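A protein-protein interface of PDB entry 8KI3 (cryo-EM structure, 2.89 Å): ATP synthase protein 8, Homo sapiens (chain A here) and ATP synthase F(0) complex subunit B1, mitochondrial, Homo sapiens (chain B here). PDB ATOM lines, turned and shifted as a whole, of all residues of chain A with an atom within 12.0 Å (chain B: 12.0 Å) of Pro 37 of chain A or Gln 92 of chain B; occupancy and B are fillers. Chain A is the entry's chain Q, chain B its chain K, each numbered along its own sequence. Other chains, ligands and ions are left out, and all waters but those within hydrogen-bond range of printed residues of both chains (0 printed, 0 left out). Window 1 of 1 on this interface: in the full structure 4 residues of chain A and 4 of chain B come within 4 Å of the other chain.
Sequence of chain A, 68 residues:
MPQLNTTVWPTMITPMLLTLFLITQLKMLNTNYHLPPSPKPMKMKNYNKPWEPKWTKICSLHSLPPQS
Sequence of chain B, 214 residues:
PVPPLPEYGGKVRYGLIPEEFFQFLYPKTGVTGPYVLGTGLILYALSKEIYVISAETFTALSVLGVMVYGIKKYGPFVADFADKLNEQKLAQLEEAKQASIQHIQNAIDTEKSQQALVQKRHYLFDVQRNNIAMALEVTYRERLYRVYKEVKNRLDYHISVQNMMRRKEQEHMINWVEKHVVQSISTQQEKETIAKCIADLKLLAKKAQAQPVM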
ATOM      1  N   ASN A  32      -3.279 -19.270  -8.270  1.00  0.00           N
ATOM      2  CA  ASN A  32      -3.848 -17.937  -8.143  1.00  0.00           C
ATOM      3  C   ASN A  32      -3.012 -17.088  -7.200  1.00  0.00           C
ATOM      4  O   ASN A  32      -2.489 -17.581  -6.197  1.00  0.00           O
ATOM      5  CB  ASN A  32      -5.289 -17.987  -7.643  1.00  0.00           C
ATOM      6  CG  ASN A  32      -6.231 -18.597  -8.650  1.00  0.00           C
ATOM      7  OD1 ASN A  32      -6.831 -19.639  -8.402  1.00  0.00           O
ATOM      8  ND2 ASN A  32      -6.363 -17.951  -9.800  1.00  0.00           N
ATOM      9  N   TYR A  33      -2.900 -15.808  -7.530  1.00  0.00           N
ATOM     10  CA  TYR A  33      -2.128 -14.839  -6.761  1.00  0.00           C
ATOM     11  C   TYR A  33      -3.100 -13.829  -6.166  1.00  0.00           C
ATOM     12  O   TYR A  33      -3.592 -12.942  -6.867  1.00  0.00           O
ATOM     13  CB  TYR A  33      -1.093 -14.153  -7.643  1.00  0.00           C
ATOM     14  CG  TYR A  33      -0.194 -15.110  -8.378  1.00  0.00           C
ATOM     15  CD1 TYR A  33       0.996 -15.533  -7.819  1.00  0.00           C
ATOM     16  CD2 TYR A  33      -0.536 -15.591  -9.629  1.00  0.00           C
ATOM     17  CE1 TYR A  33       1.817 -16.402  -8.481  1.00  0.00           C
ATOM     18  CE2 TYR A  33       0.281 -16.464 -10.297  1.00  0.00           C
ATOM     19  CZ  TYR A  33       1.455 -16.865  -9.717  1.00  0.00           C
ATOM     20  OH  TYR A  33       2.280 -17.736 -10.377  1.00  0.00           O
ATOM     21  N   HIS A  34      -3.368 -13.965  -4.874  1.00  0.00           N
ATOM     22  CA  HIS A  34      -4.286 -13.061  -4.202  1.00  0.00           C
ATOM     23  C   HIS A  34      -3.660 -11.684  -4.038  1.00  0.00           C
ATOM     24  O   HIS A  34      -2.448 -11.545  -3.862  1.00  0.00           O
ATOM     25  CB  HIS A  34      -4.666 -13.618  -2.838  1.00  0.00           C
ATOM     26  CG  HIS A  34      -3.519 -13.681  -1.884  1.00  0.00           C
ATOM     27  ND1 HIS A  34      -3.016 -12.566  -1.252  1.00  0.00           N
ATOM     28  CD2 HIS A  34      -2.766 -14.723  -1.467  1.00  0.00           C
ATOM     29  CE1 HIS A  34      -2.006 -12.921  -0.480  1.00  0.00           C
ATOM     30  NE2 HIS A  34      -1.834 -14.225  -0.592  1.00  0.00           N
ATOM     31  N   LEU A  35      -4.504 -10.659  -4.086  1.00  0.00           N
ATOM     32  CA  LEU A  35      -4.033  -9.299  -3.900  1.00  0.00           C
ATOM     33  C   LEU A  35      -3.581  -9.101  -2.455  1.00  0.00           C
ATOM     34  O   LEU A  35      -4.140  -9.703  -1.536  1.00  0.00           O
ATOM     35  CB  LEU A  35      -5.132  -8.298  -4.236  1.00  0.00           C
ATOM     36  CG  LEU A  35      -5.490  -8.081  -5.705  1.00  0.00           C
ATOM     37  CD1 LEU A  35      -6.330  -9.226  -6.236  1.00  0.00           C
ATOM     38  CD2 LEU A  35      -6.212  -6.764  -5.890  1.00  0.00           C
ATOM     39  N   PRO A  36      -2.571  -8.271  -2.223  1.00  0.00           N
ATOM     40  CA  PRO A  36      -2.071  -8.075  -0.860  1.00  0.00           C
ATOM     41  C   PRO A  36      -3.068  -7.294  -0.025  1.00  0.00           C
ATOM     42  O   PRO A  36      -3.857  -6.505  -0.563  1.00  0.00           O
ATOM     43  CB  PRO A  36      -0.772  -7.282  -1.067  1.00  0.00           C
ATOM     44  CG  PRO A  36      -0.449  -7.421  -2.520  1.00  0.00           C
ATOM     45  CD  PRO A  36      -1.764  -7.541  -3.210  1.00  0.00           C
ATOM     46  N   PRO A  37      -3.066  -7.484   1.288  1.00  0.00           N
ATOM     47  CA  PRO A  37      -3.991  -6.759   2.160  1.00  0.00           C
ATOM     48  C   PRO A  37      -3.451  -5.368   2.478  1.00  0.00           C
ATOM     49  O   PRO A  37      -2.408  -4.951   1.983  1.00  0.00           O
ATOM     50  CB  PRO A  37      -4.055  -7.637   3.416  1.00  0.00           C
ATOM     51  CG  PRO A  37      -3.254  -8.875   3.097  1.00  0.00           C
ATOM     52  CD  PRO A  37      -2.293  -8.478   2.041  1.00  0.00           C
ATOM     53  N   SER A  38      -4.189  -4.651   3.321  1.00  0.00           N
ATOM     54  CA  SER A  38      -3.785  -3.314   3.749  1.00  0.00           C
ATOM     55  C   SER A  38      -2.477  -3.355   4.527  1.00  0.00           C
ATOM     56  O   SER A  38      -1.546  -2.608   4.230  1.00  0.00           O
ATOM     57  CB  SER A  38      -4.878  -2.672   4.604  1.00  0.00           C
ATOM     58  OG  SER A  38      -5.192  -3.487   5.719  1.00  0.00           O
ATOM     59  N   ASP B  83      12.000 -20.873   1.228  1.00  0.00           N
ATOM     60  CA  ASP B  83      11.510 -20.566   2.565  1.00  0.00           C
ATOM     61  C   ASP B  83      11.313 -19.068   2.747  1.00  0.00           C
ATOM     62  O   ASP B  83      10.282 -18.629   3.265  1.00  0.00           O
ATOM     63  CB  ASP B  83      12.473 -21.108   3.616  1.00  0.00           C
ATOM     64  CG  ASP B  83      12.276 -22.578   3.871  1.00  0.00           C
ATOM     65  OD1 ASP B  83      11.117 -23.035   3.815  1.00  0.00           O
ATOM     66  OD2 ASP B  83      13.277 -23.276   4.126  1.00  0.00           O
ATOM     67  N   LYS B  84      12.296 -18.271   2.326  1.00  0.00           N
ATOM     68  CA  LYS B  84      12.183 -16.825   2.469  1.00  0.00           C
ATOM     69  C   LYS B  84      10.969 -16.276   1.737  1.00  0.00           C
ATOM     70  O   LYS B  84      10.403 -15.265   2.160  1.00  0.00           O
ATOM     71  CB  LYS B  84      13.456 -16.144   1.975  1.00  0.00           C
ATOM     72  CG  LYS B  84      14.639 -16.342   2.902  1.00  0.00           C
ATOM     73  CD  LYS B  84      15.834 -15.514   2.465  1.00  0.00           C
ATOM     74  CE  LYS B  84      17.027 -15.762   3.372  1.00  0.00           C
ATOM     75  NZ  LYS B  84      17.404 -17.201   3.413  1.00  0.00           N
ATOM     76  N   LEU B  85      10.547 -16.917   0.646  1.00  0.00           N
ATOM     77  CA  LEU B  85       9.311 -16.491  -0.001  1.00  0.00           C
ATOM     78  C   LEU B  85       8.102 -16.738   0.882  1.00  0.00           C
ATOM     79  O   LEU B  85       7.074 -16.073   0.724  1.00  0.00           O
ATOM     80  CB  LEU B  85       9.126 -17.202  -1.337  1.00  0.00           C
ATOM     81  CG  LEU B  85      10.032 -16.745  -2.466  1.00  0.00           C
ATOM     82  CD1 LEU B  85       9.814 -17.617  -3.677  1.00  0.00           C
ATOM     83  CD2 LEU B  85       9.721 -15.303  -2.787  1.00  0.00           C
ATOM     84  N   ASN B  86       8.198 -17.688   1.810  1.00  0.00           N
ATOM     85  CA  ASN B  86       7.078 -17.964   2.701  1.00  0.00           C
ATOM     86  C   ASN B  86       7.141 -17.087   3.944  1.00  0.00           C
ATOM     87  O   ASN B  86       6.188 -16.364   4.253  1.00  0.00           O
ATOM     88  CB  ASN B  86       7.063 -19.443   3.082  1.00  0.00           C
ATOM     89  CG  ASN B  86       6.403 -20.300   2.033  1.00  0.00           C
ATOM     90  OD1 ASN B  86       5.510 -19.845   1.323  1.00  0.00           O
ATOM     91  ND2 ASN B  86       6.839 -21.547   1.925  1.00  0.00           N
ATOM     92  N   GLU B  87       8.266 -17.116   4.657  1.00  0.00           N
ATOM     93  CA  GLU B  87       8.396 -16.328   5.875  1.00  0.00           C
ATOM     94  C   GLU B  87       8.377 -14.835   5.570  1.00  0.00           C
ATOM     95  O   GLU B  87       8.393 -14.010   6.487  1.00  0.00           O
ATOM     96  CB  GLU B  87       9.665 -16.713   6.634  1.00  0.00           C
ATOM     97  CG  GLU B  87      10.920 -15.998   6.189  1.00  0.00           C
ATOM     98  CD  GLU B  87      12.157 -16.524   6.889  1.00  0.00           C
ATOM     99  OE1 GLU B  87      12.035 -17.515   7.640  1.00  0.00           O
ATOM    100  OE2 GLU B  87      13.249 -15.955   6.687  1.00  0.00           O
ATOM    101  N   GLN B  88       8.348 -14.476   4.288  1.00  0.00           N
ATOM    102  CA  GLN B  88       7.976 -13.124   3.898  1.00  0.00           C
ATOM    103  C   GLN B  88       6.469 -13.004   3.724  1.00  0.00           C
ATOM    104  O   GLN B  88       5.841 -12.127   4.322  1.00  0.00           O
ATOM    105  CB  GLN B  88       8.681 -12.717   2.605  1.00  0.00           C
ATOM    106  CG  GLN B  88      10.084 -12.183   2.793  1.00  0.00           C
ATOM    107  CD  GLN B  88      10.730 -11.806   1.478  1.00  0.00           C
ATOM    108  OE1 GLN B  88      11.953 -11.779   1.358  1.00  0.00           O
ATOM    109  NE2 GLN B  88       9.905 -11.510   0.479  1.00  0.00           N
ATOM    110  N   LYS B  89       5.879 -13.879   2.909  1.00  0.00           N
ATOM    111  CA  LYS B  89       4.434 -13.850   2.722  1.00  0.00           C
ATOM    112  C   LYS B  89       3.700 -14.118   4.024  1.00  0.00           C
ATOM    113  O   LYS B  89       2.597 -13.603   4.233  1.00  0.00           O
ATOM    114  CB  LYS B  89       4.023 -14.867   1.660  1.00  0.00           C
ATOM    115  CG  LYS B  89       2.534 -14.920   1.389  1.00  0.00           C
ATOM    116  CD  LYS B  89       2.206 -16.035   0.418  1.00  0.00           C
ATOM    117  CE  LYS B  89       0.712 -16.169   0.213  1.00  0.00           C
ATOM    118  NZ  LYS B  89       0.378 -17.354  -0.622  1.00  0.00           N
ATOM    119  N   LEU B  90       4.291 -14.912   4.913  1.00  0.00           N
ATOM    120  CA  LEU B  90       3.694 -15.111   6.227  1.00  0.00           C
ATOM    121  C   LEU B  90       3.750 -13.829   7.047  1.00  0.00           C
ATOM    122  O   LEU B  90       2.728 -13.366   7.565  1.00  0.00           O
ATOM    123  CB  LEU B  90       4.402 -16.250   6.954  1.00  0.00           C
ATOM    124  CG  LEU B  90       3.953 -16.511   8.387  1.00  0.00           C
ATOM    125  CD1 LEU B  90       2.512 -16.967   8.403  1.00  0.00           C
ATOM    126  CD2 LEU B  90       4.851 -17.544   9.039  1.00  0.00           C
ATOM    127  N   ALA B  91       4.941 -13.237   7.168  1.00  0.00           N
ATOM    128  CA  ALA B  91       5.085 -12.008   7.939  1.00  0.00           C
ATOM    129  C   ALA B  91       4.270 -10.874   7.334  1.00  0.00           C
ATOM    130  O   ALA B  91       3.665 -10.081   8.063  1.00  0.00           O
ATOM    131  CB  ALA B  91       6.559 -11.617   8.031  1.00  0.00           C
ATOM    132  N   GLN B  92       4.247 -10.776   6.004  1.00  0.00           N
ATOM    133  CA  GLN B  92       3.448  -9.751   5.342  1.00  0.00           C
ATOM    134  C   GLN B  92       1.974  -9.846   5.708  1.00  0.00           C
ATOM    135  O   GLN B  92       1.263  -8.838   5.645  1.00  0.00           O
ATOM    136  CB  GLN B  92       3.627  -9.856   3.827  1.00  0.00           C
ATOM    137  CG  GLN B  92       2.749  -8.924   3.013  1.00  0.00           C
ATOM    138  CD  GLN B  92       2.493  -9.446   1.614  1.00  0.00           C
ATOM    139  OE1 GLN B  92       3.307 -10.181   1.058  1.00  0.00           O
ATOM    140  NE2 GLN B  92       1.357  -9.070   1.040  1.00  0.00           N
ATOM    141  N   LEU B  93       1.499 -11.025   6.106  1.00  0.00           N
ATOM    142  CA  LEU B  93       0.112 -11.157   6.532  1.00  0.00           C
ATOM    143  C   LEU B  93      -0.043 -10.821   8.010  1.00  0.00           C
ATOM    144  O   LEU B  93      -0.863  -9.974   8.381  1.00  0.00           O
ATOM    145  CB  LEU B  93      -0.398 -12.569   6.241  1.00  0.00           C
ATOM    146  CG  LEU B  93      -0.591 -12.921   4.769  1.00  0.00           C
ATOM    147  CD1 LEU B  93      -1.255 -14.272   4.636  1.00  0.00           C
ATOM    148  CD2 LEU B  93      -1.411 -11.856   4.078  1.00  0.00           C
ATOM    149  N   GLU B  94       0.737 -11.482   8.869  1.00  0.00           N
ATOM    150  CA  GLU B  94       0.645 -11.238  10.304  1.00  0.00           C
ATOM    151  C   GLU B  94       0.815  -9.767  10.642  1.00  0.00           C
ATOM    152  O   GLU B  94       0.198  -9.272  11.590  1.00  0.00           O
ATOM    153  CB  GLU B  94       1.690 -12.068  11.049  1.00  0.00           C
ATOM    154  CG  GLU B  94       1.571 -13.564  10.836  1.00  0.00           C
ATOM    155  CD  GLU B  94       0.445 -14.189  11.635  1.00  0.00           C
ATOM    156  OE1 GLU B  94      -0.307 -13.446  12.298  1.00  0.00           O
ATOM    157  OE2 GLU B  94       0.316 -15.431  11.606  1.00  0.00           O
ATOM    158  N   GLU B  95       1.642  -9.069   9.859  1.00  0.00           N
ATOM    159  CA  GLU B  95       1.858  -7.615  10.081  1.00  0.00           C
ATOM    160  C   GLU B  95       0.544  -6.869   9.830  1.00  0.00           C
ATOM    161  O   GLU B  95       0.017  -6.263  10.784  1.00  0.00           O
ATOM    162  CB  GLU B  95       2.957  -7.095   9.153  1.00  0.00           C
ATOM    163  CG  GLU B  95       3.173  -5.597   9.255  1.00  0.00           C
ATOM    164  CD  GLU B  95       4.206  -5.043   8.291  1.00  0.00           C
ATOM    165  OE1 GLU B  95       4.774  -5.836   7.515  1.00  0.00           O
ATOM    166  OE2 GLU B  95       4.442  -3.819   8.320  1.00  0.00           O
ATOM    167  N   ALA B  96       0.036  -6.924   8.595  1.00  0.00           N
ATOM    168  CA  ALA B  96      -1.222  -6.223   8.248  1.00  0.00           C
ATOM    169  C   ALA B  96      -2.342  -6.704   9.176  1.00  0.00           C
ATOM    170  O   ALA B  96      -3.202  -5.881   9.542  1.00  0.00           O
ATOM    171  CB  ALA B  96      -1.564  -6.468   6.799  1.00  0.00           C
ATOM    172  N   LYS B  97      -2.320  -7.989   9.543  1.00  0.00           N
ATOM    173  CA  LYS B  97      -3.364  -8.556  10.435  1.00  0.00           C
ATOM    174  C   LYS B  97      -3.417  -7.737  11.730  1.00  0.00           C
ATOM    175  O   LYS B  97      -4.533  -7.367  12.147  1.00  0.00           O
ATOM    176  CB  LYS B  97      -3.056 -10.027  10.729  1.00  0.00           C
ATOM    177  CG  LYS B  97      -3.925 -10.680  11.794  1.00  0.00           C
ATOM    178  CD  LYS B  97      -3.543 -12.119  12.067  1.00  0.00           C
ATOM    179  CE  LYS B  97      -4.316 -12.730  13.217  1.00  0.00           C
ATOM    180  NZ  LYS B  97      -5.778 -12.656  12.992  1.00  0.00           N
ATOM    181  N   GLN B  98      -2.256  -7.461  12.329  1.00  0.00           N
ATOM    182  CA  GLN B  98      -2.204  -6.670  13.589  1.00  0.00           C
ATOM    183  C   GLN B  98      -2.640  -5.231  13.297  1.00  0.00           C
ATOM    184  O   GLN B  98      -3.450  -4.691  14.074  1.00  0.00           O
ATOM    185  CB  GLN B  98      -0.798  -6.703  14.187  1.00  0.00           C
ATOM    186  CG  GLN B  98      -0.214  -8.105  14.290  1.00  0.00           C
ATOM    187  CD  GLN B  98      -1.230  -9.116  14.761  1.00  0.00           C
ATOM    188  OE1 GLN B  98      -1.789  -9.005  15.850  1.00  0.00           O
ATOM    189  NE2 GLN B  98      -1.479 -10.119  13.934  1.00  0.00           N
ATOM    190  N   ALA B  99      -2.118  -4.639  12.219  1.00  0.00           N
ATOM    191  CA  ALA B  99      -2.501  -3.259  11.841  1.00  0.00           C
ATOM    192  C   ALA B  99      -4.023  -3.188  11.695  1.00  0.00           C
ATOM    193  O   ALA B  99      -4.627  -2.244  12.244  1.00  0.00           O
ATOM    194  CB  ALA B  99      -1.804  -2.864  10.564  1.00  0.00           C
ATOM    195  N   SER B 100      -4.614  -4.151  10.983  1.00  0.00           N
ATOM    196  CA  SER B 100      -6.056  -4.179  10.809  1.00  0.00           C
ATOM    197  C   SER B 100      -6.805  -4.203  12.129  1.00  0.00           C
ATOM    198  O   SER B 100      -8.030  -4.045  12.132  1.00  0.00           O
ATOM    199  CB  SER B 100      -6.480  -5.387   9.974  1.00  0.00           C
ATOM    200  OG  SER B 100      -7.882  -5.569  10.044  1.00  0.00           O
ATOM    201  N   ILE B 101      -6.106  -4.405  13.246  1.00  0.00           N
ATOM    202  CA  ILE B 101      -6.739  -4.249  14.552  1.00  0.00           C
ATOM    203  C   ILE B 101      -6.689  -2.792  14.990  1.00  0.00           C
ATOM    204  O   ILE B 101      -7.677  -2.244  15.489  1.00  0.00           O
ATOM    205  CB  ILE B 101      -6.079  -5.176  15.585  1.00  0.00           C
ATOM    206  CG1 ILE B 101      -6.346  -6.634  15.232  1.00  0.00           C
ATOM    207  CG2 ILE B 101      -6.589  -4.873  16.973  1.00  0.00           C
ATOM    208  CD1 ILE B 101      -5.564  -7.610  16.075  1.00  0.00           C
ATOM    209  N   HIS B 103      -6.697  -0.199  13.136  1.00  0.00           N
ATOM    210  CA  HIS B 103      -7.748   0.498  12.410  1.00  0.00           C
ATOM    211  C   HIS B 103      -9.137   0.144  12.916  1.00  0.00           C
ATOM    212  O   HIS B 103     -10.107   0.788  12.505  1.00  0.00           O
ATOM    213  CB  HIS B 103      -7.651   0.194  10.916  1.00  0.00           C
ATOM    214  CG  HIS B 103      -8.279   1.236  10.042  1.00  0.00           C
ATOM    215  ND1 HIS B 103      -7.572   2.304   9.532  1.00  0.00           N
ATOM    216  CD2 HIS B 103      -9.547   1.375   9.587  1.00  0.00           C
ATOM    217  CE1 HIS B 103      -8.376   3.052   8.798  1.00  0.00           C
ATOM    218  NE2 HIS B 103      -9.580   2.511   8.817  1.00  0.00           N
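Among the printed residues, pairs that only touch across the chains: His 34 of chain A with Lys 89 of chain B (3.3 Å), Pro 36 of chain A with Gln 92 of chain B (3.5 Å), Pro 37 of chain A with Gln 92 of chain B (3.8 Å), Pro 37 of chain A with Leu 93 of chain B (3.6 Å) and Ser 38 of chain A with Ala 96 of chain B (3.96 Å).
Printed residues of chain B within 4 Å of His 34 of chain A: Lys 89 (3.3 Å). Of chain B, only Gln 92 (3.8 Å) and Leu 93 (3.6 Å) come within 4 Å of Pro 37 of chain A. Ser 38 of chain A touches just one residue of chain B: Ala 96 (3.96 Å). Asp 83 of chain B touches none of the printed residues of chain A. Lys 84 of chain B touches none of the printed residues of chain A. Lys 89 of chain B touches just one residue of chain A: His 34 (3.3 Å). Leu 90 of chain B touches none of the printed residues of chain A. No residue of chain A comes within 4 Å of Ala 91 of chain B. Gln 92 of chain B touches just these residues of chain A: Pro 36 (3.5 Å) and Pro 37 (3.8 Å). Of the printed residues of chain A, Leu 93 of chain B touches Pro 37. No residue of chain A comes within 4 Å of Glu 95 of chain B. The nearest residue of chain A that does not touch Gln 92 of chain B is His 34 of chain A (5.3 Å).
Printed residues of chain A that touch a printed residue of chain B: His 34, Pro 36, Pro 37 and Ser 38. Printed residues of chain B that touch a printed residue of chain A: Lys 89, Gln 92, Leu 93 and Ala 96. Hydrophobic or aromatic side chains of chain B within 4 Å of the printed part of chain A: Leu 93 and Ala 96. Among the printed residues, 5 pairs touch across the chains. Among the printed residues, no Asp or Glu carboxylate lies within 4 Å of a Lys or Arg side-chain nitrogen of the other chain.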
